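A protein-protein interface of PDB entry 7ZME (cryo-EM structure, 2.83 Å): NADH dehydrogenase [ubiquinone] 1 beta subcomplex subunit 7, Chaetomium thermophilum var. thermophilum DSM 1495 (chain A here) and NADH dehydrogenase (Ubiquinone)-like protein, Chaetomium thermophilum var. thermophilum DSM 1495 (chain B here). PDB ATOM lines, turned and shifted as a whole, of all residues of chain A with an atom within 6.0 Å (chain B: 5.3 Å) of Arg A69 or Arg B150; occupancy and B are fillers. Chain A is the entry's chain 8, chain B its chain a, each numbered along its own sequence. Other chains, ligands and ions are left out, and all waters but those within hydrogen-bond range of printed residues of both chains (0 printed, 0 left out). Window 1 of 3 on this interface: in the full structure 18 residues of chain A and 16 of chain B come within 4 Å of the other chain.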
ATOM      1  N   ALA A  25      31.176  10.753  16.184  1.00  0.00           N
ATOM      2  CA  ALA A  25      29.782  11.169  16.140  1.00  0.00           C
ATOM      3  C   ALA A  25      28.844  10.117  16.705  1.00  0.00           C
ATOM      4  O   ALA A  25      27.662  10.411  16.916  1.00  0.00           O
ATOM      5  CB  ALA A  25      29.381  11.507  14.707  1.00  0.00           C
ATOM      6  N   TYR A  26      29.335   8.904  16.950  1.00  0.00           N
ATOM      7  CA  TYR A  26      28.536   7.822  17.501  1.00  0.00           C
ATOM      8  C   TYR A  26      28.979   7.455  18.913  1.00  0.00           C
ATOM      9  O   TYR A  26      28.641   6.377  19.410  1.00  0.00           O
ATOM     10  CB  TYR A  26      28.606   6.615  16.569  1.00  0.00           C
ATOM     11  CG  TYR A  26      27.949   6.888  15.239  1.00  0.00           C
ATOM     12  CD1 TYR A  26      26.943   7.838  15.125  1.00  0.00           C
ATOM     13  CD2 TYR A  26      28.376   6.246  14.088  1.00  0.00           C
ATOM     14  CE1 TYR A  26      26.353   8.110  13.913  1.00  0.00           C
ATOM     15  CE2 TYR A  26      27.794   6.516  12.868  1.00  0.00           C
ATOM     16  CZ  TYR A  26      26.781   7.447  12.787  1.00  0.00           C
ATOM     17  OH  TYR A  26      26.198   7.716  11.572  1.00  0.00           O
ATOM     18  N   ARG A  27      29.733   8.339  19.565  1.00  0.00           N
ATOM     19  CA  ARG A  27      30.153   8.147  20.951  1.00  0.00           C
ATOM     20  C   ARG A  27      29.017   8.580  21.872  1.00  0.00           C
ATOM     21  O   ARG A  27      29.013   9.672  22.445  1.00  0.00           O
ATOM     22  CB  ARG A  27      31.427   8.924  21.248  1.00  0.00           C
ATOM     23  CG  ARG A  27      32.639   8.539  20.423  1.00  0.00           C
ATOM     24  CD  ARG A  27      33.549   7.604  21.185  1.00  0.00           C
ATOM     25  NE  ARG A  27      34.486   6.927  20.300  1.00  0.00           N
ATOM     26  CZ  ARG A  27      35.769   7.244  20.185  1.00  0.00           C
ATOM     27  NH1 ARG A  27      36.279   8.230  20.908  1.00  0.00           N
ATOM     28  NH2 ARG A  27      36.544   6.567  19.350  1.00  0.00           N
ATOM     29  N   ASP A  28      28.031   7.698  22.019  1.00  0.00           N
ATOM     30  CA  ASP A  28      26.897   8.006  22.881  1.00  0.00           C
ATOM     31  C   ASP A  28      26.422   6.774  23.642  1.00  0.00           C
ATOM     32  O   ASP A  28      27.109   5.748  23.668  1.00  0.00           O
ATOM     33  CB  ASP A  28      25.760   8.615  22.059  1.00  0.00           C
ATOM     34  CG  ASP A  28      25.074   7.605  21.173  1.00  0.00           C
ATOM     35  OD1 ASP A  28      25.773   6.760  20.576  1.00  0.00           O
ATOM     36  OD2 ASP A  28      23.832   7.670  21.063  1.00  0.00           O
ATOM     37  N   CYS A  30      23.948   4.521  23.312  1.00  0.00           N
ATOM     38  CA  CYS A  30      23.609   3.295  22.600  1.00  0.00           C
ATOM     39  C   CYS A  30      24.817   2.582  22.011  1.00  0.00           C
ATOM     40  O   CYS A  30      24.674   1.437  21.572  1.00  0.00           O
ATOM     41  CB  CYS A  30      22.609   3.605  21.488  1.00  0.00           C
ATOM     42  SG  CYS A  30      23.221   4.806  20.303  1.00  0.00           S
ATOM     43  N   GLN A  62      18.592   2.916  18.296  1.00  0.00           N
ATOM     44  CA  GLN A  62      18.644   4.216  17.639  1.00  0.00           C
ATOM     45  C   GLN A  62      17.278   4.883  17.643  1.00  0.00           C
ATOM     46  O   GLN A  62      17.176   6.099  17.837  1.00  0.00           O
ATOM     47  CB  GLN A  62      19.124   4.062  16.195  1.00  0.00           C
ATOM     48  CG  GLN A  62      20.541   3.553  16.012  1.00  0.00           C
ATOM     49  CD  GLN A  62      21.585   4.488  16.570  1.00  0.00           C
ATOM     50  OE1 GLN A  62      22.207   4.195  17.585  1.00  0.00           O
ATOM     51  NE2 GLN A  62      21.786   5.619  15.909  1.00  0.00           N
ATOM     52  N   LEU A  64      14.577   4.399  19.702  1.00  0.00           N
ATOM     53  CA  LEU A  64      14.065   4.789  21.013  1.00  0.00           C
ATOM     54  C   LEU A  64      14.710   6.077  21.505  1.00  0.00           C
ATOM     55  O   LEU A  64      14.018   6.975  21.999  1.00  0.00           O
ATOM     56  CB  LEU A  64      14.282   3.664  22.027  1.00  0.00           C
ATOM     57  CG  LEU A  64      13.266   2.518  22.090  1.00  0.00           C
ATOM     58  CD1 LEU A  64      11.904   3.045  22.518  1.00  0.00           C
ATOM     59  CD2 LEU A  64      13.164   1.752  20.779  1.00  0.00           C
ATOM     60  N   GLU A  65      16.036   6.185  21.389  1.00  0.00           N
ATOM     61  CA  GLU A  65      16.701   7.421  21.788  1.00  0.00           C
ATOM     62  C   GLU A  65      16.286   8.581  20.899  1.00  0.00           C
ATOM     63  O   GLU A  65      16.200   9.721  21.365  1.00  0.00           O
ATOM     64  CB  GLU A  65      18.218   7.241  21.760  1.00  0.00           C
ATOM     65  CG  GLU A  65      18.992   8.396  22.378  1.00  0.00           C
ATOM     66  CD  GLU A  65      18.700   8.577  23.855  1.00  0.00           C
ATOM     67  OE1 GLU A  65      18.394   7.571  24.532  1.00  0.00           O
ATOM     68  OE2 GLU A  65      18.776   9.725  24.342  1.00  0.00           O
ATOM     69  N   PHE A  66      16.030   8.308  19.618  1.00  0.00           N
ATOM     70  CA  PHE A  66      15.494   9.335  18.734  1.00  0.00           C
ATOM     71  C   PHE A  66      14.117   9.788  19.196  1.00  0.00           C
ATOM     72  O   PHE A  66      13.817  10.987  19.193  1.00  0.00           O
ATOM     73  CB  PHE A  66      15.433   8.805  17.301  1.00  0.00           C
ATOM     74  CG  PHE A  66      14.820   9.765  16.326  1.00  0.00           C
ATOM     75  CD1 PHE A  66      15.548  10.835  15.842  1.00  0.00           C
ATOM     76  CD2 PHE A  66      13.514   9.603  15.901  1.00  0.00           C
ATOM     77  CE1 PHE A  66      14.987  11.720  14.947  1.00  0.00           C
ATOM     78  CE2 PHE A  66      12.948  10.486  15.012  1.00  0.00           C
ATOM     79  CZ  PHE A  66      13.685  11.545  14.534  1.00  0.00           C
ATOM     80  N   LYS A  67      13.265   8.840  19.595  1.00  0.00           N
ATOM     81  CA  LYS A  67      11.923   9.187  20.054  1.00  0.00           C
ATOM     82  C   LYS A  67      11.970  10.014  21.332  1.00  0.00           C
ATOM     83  O   LYS A  67      11.174  10.943  21.506  1.00  0.00           O
ATOM     84  CB  LYS A  67      11.091   7.925  20.264  1.00  0.00           C
ATOM     85  CG  LYS A  67      10.295   7.504  19.043  1.00  0.00           C
ATOM     86  CD  LYS A  67       9.162   8.477  18.763  1.00  0.00           C
ATOM     87  CE  LYS A  67       8.397   8.086  17.510  1.00  0.00           C
ATOM     88  NZ  LYS A  67       7.631   6.824  17.698  1.00  0.00           N
ATOM     89  N   LYS A  68      12.881   9.683  22.246  1.00  0.00           N
ATOM     90  CA  LYS A  68      13.038  10.503  23.439  1.00  0.00           C
ATOM     91  C   LYS A  68      13.568  11.891  23.114  1.00  0.00           C
ATOM     92  O   LYS A  68      13.387  12.813  23.914  1.00  0.00           O
ATOM     93  CB  LYS A  68      13.959   9.803  24.440  1.00  0.00           C
ATOM     94  CG  LYS A  68      13.359   8.541  25.034  1.00  0.00           C
ATOM     95  CD  LYS A  68      14.292   7.896  26.042  1.00  0.00           C
ATOM     96  CE  LYS A  68      13.683   6.623  26.607  1.00  0.00           C
ATOM     97  NZ  LYS A  68      14.583   5.962  27.591  1.00  0.00           N
ATOM     98  N   ARG A  69      14.213  12.062  21.960  1.00  0.00           N
ATOM     99  CA  ARG A  69      14.703  13.371  21.554  1.00  0.00           C
ATOM    100  C   ARG A  69      13.719  14.139  20.680  1.00  0.00           C
ATOM    101  O   ARG A  69      13.975  15.307  20.373  1.00  0.00           O
ATOM    102  CB  ARG A  69      16.040  13.237  20.819  1.00  0.00           C
ATOM    103  CG  ARG A  69      17.191  12.781  21.706  1.00  0.00           C
ATOM    104  CD  ARG A  69      18.503  12.740  20.941  1.00  0.00           C
ATOM    105  NE  ARG A  69      18.520  11.680  19.941  1.00  0.00           N
ATOM    106  CZ  ARG A  69      18.544  11.895  18.630  1.00  0.00           C
ATOM    107  NH1 ARG A  69      18.557  10.871  17.792  1.00  0.00           N
ATOM    108  NH2 ARG A  69      18.549  13.132  18.156  1.00  0.00           N
ATOM    109  N   VAL A  70      12.614  13.522  20.267  1.00  0.00           N
ATOM    110  CA  VAL A  70      11.590  14.264  19.540  1.00  0.00           C
ATOM    111  C   VAL A  70      10.433  14.647  20.458  1.00  0.00           C
ATOM    112  O   VAL A  70       9.754  15.649  20.213  1.00  0.00           O
ATOM    113  CB  VAL A  70      11.082  13.468  18.324  1.00  0.00           C
ATOM    114  CG1 VAL A  70      12.211  13.208  17.343  1.00  0.00           C
ATOM    115  CG2 VAL A  70      10.420  12.175  18.752  1.00  0.00           C
ATOM    116  N   GLN A  71      10.196  13.866  21.513  1.00  0.00           N
ATOM    117  CA  GLN A  71       9.174  14.194  22.497  1.00  0.00           C
ATOM    118  C   GLN A  71       9.600  15.332  23.413  1.00  0.00           C
ATOM    119  O   GLN A  71       8.738  15.969  24.028  1.00  0.00           O
ATOM    120  CB  GLN A  71       8.836  12.935  23.307  1.00  0.00           C
ATOM    121  CG  GLN A  71       7.648  13.043  24.257  1.00  0.00           C
ATOM    122  CD  GLN A  71       8.025  13.608  25.613  1.00  0.00           C
ATOM    123  OE1 GLN A  71       9.151  13.437  26.078  1.00  0.00           O
ATOM    124  NE2 GLN A  71       7.081  14.284  26.256  1.00  0.00           N
ATOM    125  N   LYS A  72      10.899  15.626  23.490  1.00  0.00           N
ATOM    126  CA  LYS A  72      11.386  16.640  24.413  1.00  0.00           C
ATOM    127  C   LYS A  72      11.053  18.058  23.967  1.00  0.00           C
ATOM    128  O   LYS A  72      11.185  18.990  24.768  1.00  0.00           O
ATOM    129  CB  LYS A  72      12.898  16.490  24.604  1.00  0.00           C
ATOM    130  CG  LYS A  72      13.415  17.051  25.920  1.00  0.00           C
ATOM    131  CD  LYS A  72      14.741  16.418  26.313  1.00  0.00           C
ATOM    132  CE  LYS A  72      15.896  17.017  25.531  1.00  0.00           C
ATOM    133  NZ  LYS A  72      16.188  18.414  25.951  1.00  0.00           N
ATOM    134  N   MET A  73      10.632  18.251  22.718  1.00  0.00           N
ATOM    135  CA  MET A  73      10.160  19.561  22.288  1.00  0.00           C
ATOM    136  C   MET A  73       8.654  19.726  22.419  1.00  0.00           C
ATOM    137  O   MET A  73       8.156  20.841  22.231  1.00  0.00           O
ATOM    138  CB  MET A  73      10.561  19.842  20.840  1.00  0.00           C
ATOM    139  CG  MET A  73      12.009  20.223  20.670  1.00  0.00           C
ATOM    140  SD  MET A  73      13.020  18.764  20.890  1.00  0.00           S
ATOM    141  CE  MET A  73      12.643  17.969  19.342  1.00  0.00           C
ATOM    142  N   VAL B 146      13.058  18.226  13.993  1.00  0.00           N
ATOM    143  CA  VAL B 146      12.210  17.184  14.552  1.00  0.00           C
ATOM    144  C   VAL B 146      12.756  16.652  15.871  1.00  0.00           C
ATOM    145  O   VAL B 146      11.986  16.329  16.775  1.00  0.00           O
ATOM    146  CB  VAL B 146      12.026  16.049  13.521  1.00  0.00           C
ATOM    147  CG1 VAL B 146      11.351  14.845  14.155  1.00  0.00           C
ATOM    148  CG2 VAL B 146      11.215  16.547  12.340  1.00  0.00           C
ATOM    149  N   SER B 147      14.075  16.565  16.013  1.00  0.00           N
ATOM    150  CA  SER B 147      14.686  15.951  17.180  1.00  0.00           C
ATOM    151  C   SER B 147      15.581  16.946  17.906  1.00  0.00           C
ATOM    152  O   SER B 147      16.180  17.832  17.292  1.00  0.00           O
ATOM    153  CB  SER B 147      15.506  14.716  16.792  1.00  0.00           C
ATOM    154  OG  SER B 147      16.624  15.075  15.999  1.00  0.00           O
ATOM    155  N   TYR B 148      15.656  16.791  19.223  1.00  0.00           N
ATOM    156  CA  TYR B 148      16.548  17.606  20.024  1.00  0.00           C
ATOM    157  C   TYR B 148      18.001  17.277  19.689  1.00  0.00           C
ATOM    158  O   TYR B 148      18.317  16.142  19.321  1.00  0.00           O
ATOM    159  CB  TYR B 148      16.298  17.370  21.510  1.00  0.00           C
ATOM    160  CG  TYR B 148      16.863  18.439  22.412  1.00  0.00           C
ATOM    161  CD1 TYR B 148      16.187  19.632  22.615  1.00  0.00           C
ATOM    162  CD2 TYR B 148      18.075  18.254  23.060  1.00  0.00           C
ATOM    163  CE1 TYR B 148      16.700  20.611  23.442  1.00  0.00           C
ATOM    164  CE2 TYR B 148      18.597  19.227  23.887  1.00  0.00           C
ATOM    165  CZ  TYR B 148      17.906  20.404  24.076  1.00  0.00           C
ATOM    166  OH  TYR B 148      18.423  21.376  24.900  1.00  0.00           O
ATOM    167  N   PRO B 149      18.897  18.257  19.783  1.00  0.00           N
ATOM    168  CA  PRO B 149      20.315  17.977  19.543  1.00  0.00           C
ATOM    169  C   PRO B 149      20.801  16.844  20.429  1.00  0.00           C
ATOM    170  O   PRO B 149      20.520  16.805  21.627  1.00  0.00           O
ATOM    171  CB  PRO B 149      21.006  19.301  19.887  1.00  0.00           C
ATOM    172  CG  PRO B 149      19.931  20.333  19.979  1.00  0.00           C
ATOM    173  CD  PRO B 149      18.601  19.696  19.744  1.00  0.00           C
ATOM    174  N   ARG B 150      21.530  15.911  19.825  1.00  0.00           N
ATOM    175  CA  ARG B 150      21.959  14.719  20.541  1.00  0.00           C
ATOM    176  C   ARG B 150      22.826  15.094  21.732  1.00  0.00           C
ATOM    177  O   ARG B 150      23.775  15.875  21.608  1.00  0.00           O
ATOM    178  CB  ARG B 150      22.725  13.793  19.602  1.00  0.00           C
ATOM    179  CG  ARG B 150      21.882  13.199  18.495  1.00  0.00           C
ATOM    180  CD  ARG B 150      22.727  12.317  17.600  1.00  0.00           C
ATOM    181  NE  ARG B 150      23.209  11.134  18.306  1.00  0.00           N
ATOM    182  CZ  ARG B 150      24.099  10.284  17.809  1.00  0.00           C
ATOM    183  NH1 ARG B 150      24.483   9.233  18.520  1.00  0.00           N
ATOM    184  NH2 ARG B 150      24.608  10.486  16.601  1.00  0.00           N
ATOM    185  N   GLU B 151      22.491  14.541  22.892  1.00  0.00           N
ATOM    186  CA  GLU B 151      23.300  14.731  24.082  1.00  0.00           C
ATOM    187  C   GLU B 151      24.518  13.823  24.025  1.00  0.00           C
ATOM    188  O   GLU B 151      24.435  12.674  23.585  1.00  0.00           O
ATOM    189  CB  GLU B 151      22.482  14.442  25.340  1.00  0.00           C
ATOM    190  CG  GLU B 151      23.207  14.760  26.636  1.00  0.00           C
ATOM    191  CD  GLU B 151      23.189  16.238  26.965  1.00  0.00           C
ATOM    192  OE1 GLU B 151      22.253  16.935  26.523  1.00  0.00           O
ATOM    193  OE2 GLU B 151      24.116  16.703  27.661  1.00  0.00           O
ATOM    194  N   PHE B 152      25.655  14.345  24.471  1.00  0.00           N
ATOM    195  CA  PHE B 152      26.907  13.601  24.489  1.00  0.00           C
ATOM    196  C   PHE B 152      27.471  13.629  25.901  1.00  0.00           C
ATOM    197  O   PHE B 152      27.641  14.707  26.481  1.00  0.00           O
ATOM    198  CB  PHE B 152      27.900  14.188  23.490  1.00  0.00           C
ATOM    199  CG  PHE B 152      27.542  13.921  22.057  1.00  0.00           C
ATOM    200  CD1 PHE B 152      27.655  12.647  21.529  1.00  0.00           C
ATOM    201  CD2 PHE B 152      27.089  14.942  21.242  1.00  0.00           C
ATOM    202  CE1 PHE B 152      27.330  12.398  20.217  1.00  0.00           C
ATOM    203  CE2 PHE B 152      26.760  14.699  19.929  1.00  0.00           C
ATOM    204  CZ  PHE B 152      26.880  13.424  19.414  1.00  0.00           C
ATOM    205  N   PHE B 169      27.862  18.364  21.901  1.00  0.00           N
ATOM    206  CA  PHE B 169      26.717  18.928  22.604  1.00  0.00           C
ATOM    207  C   PHE B 169      26.600  18.323  23.998  1.00  0.00           C
ATOM    208  O   PHE B 169      26.558  17.099  24.148  1.00  0.00           O
ATOM    209  CB  PHE B 169      25.441  18.671  21.802  1.00  0.00           C
ATOM    210  CG  PHE B 169      24.354  19.680  22.037  1.00  0.00           C
ATOM    211  CD1 PHE B 169      24.417  20.934  21.452  1.00  0.00           C
ATOM    212  CD2 PHE B 169      23.268  19.372  22.836  1.00  0.00           C
ATOM    213  CE1 PHE B 169      23.416  21.863  21.663  1.00  0.00           C
ATOM    214  CE2 PHE B 169      22.264  20.297  23.052  1.00  0.00           C
ATOM    215  CZ  PHE B 169      22.339  21.544  22.464  1.00  0.00           C
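The side-chain sulfur (SG) of Cys A30 is in hydrogen-bond range of the side-chain carboxylate (OD2) of Asp A28 (3.0 Å).
The backbone NH of Phe B152 sits at hydrogen-bond distance from the backbone carbonyl oxygen of Phe B169, 2.9 Å away.
The backbone carbonyl oxygen of Glu A65 lies close to the guanidinium group of Arg A69.
Of the printed residues of chain B, Asp A28 touches Arg B150 (3.1 Å).
Of the printed residues of chain B, Phe A66 touches Ser B147 (3.6 Å).
Of the printed residues of chain B, Arg A69 touches Ser B147, Tyr B148 and Arg B150.
Printed residues of chain B within 4 Å of Lys A72: Tyr B148.
Printed residues of chain A within 4 Å of Val B146: Val A70 and Met A73.
Printed residues of chain A within 4 Å of Ser B147: Phe A66, Arg A69, Val A70 and Met A73.
The nearest residue of chain B that does not touch Arg A69 is Val B146 (4.2 Å).
The nearest residue of chain A that does not touch Arg B150 is Cys A30 (4.9 Å).
Phe B152 touches Ala A25 (CE1 to O, 3.9 Å).
Tyr A26 touches Arg B150.
O of Arg A27 touches CD1 of Phe B152 (3.4 Å).
Ser B147 touches Phe A66.
Arg B150 touches Arg A69.
O of Val B146 touches CG1 of Val A70, 3.2 Å away.
Ser B147 touches Val A70.
CZ of Tyr B148 touches NZ of Lys A72, 3.2 Å away.
Met A73 touches Val B146.
Met A73 touches Ser B147.
Printed residues of chain B that touch a printed residue of chain A: Val B146, Ser B147, Tyr B148, Arg B150 and Phe B152.
Along chain B the printed residues that touch a printed residue of chain A span positions 146 to 152.
N of Tyr B148 is in hydrogen-bond range of O of Arg A69, 2.5 Å away.
OG of Ser B147 lies within hydrogen-bond range of NH2 of Arg A69 (3.5 Å).
N of Tyr B148 lies close to SD of Met A73 (3.7 Å).
The side-chain carboxylate (OD2) of Asp A28 lies within salt-bridge range of the guanidinium group (NH1) of Arg B150.
The backbone carbonyl oxygen (O) of Ala A25 sits at hydrogen-bond distance from the guanidinium group (NH2) of Arg B150 (3.1 Å).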
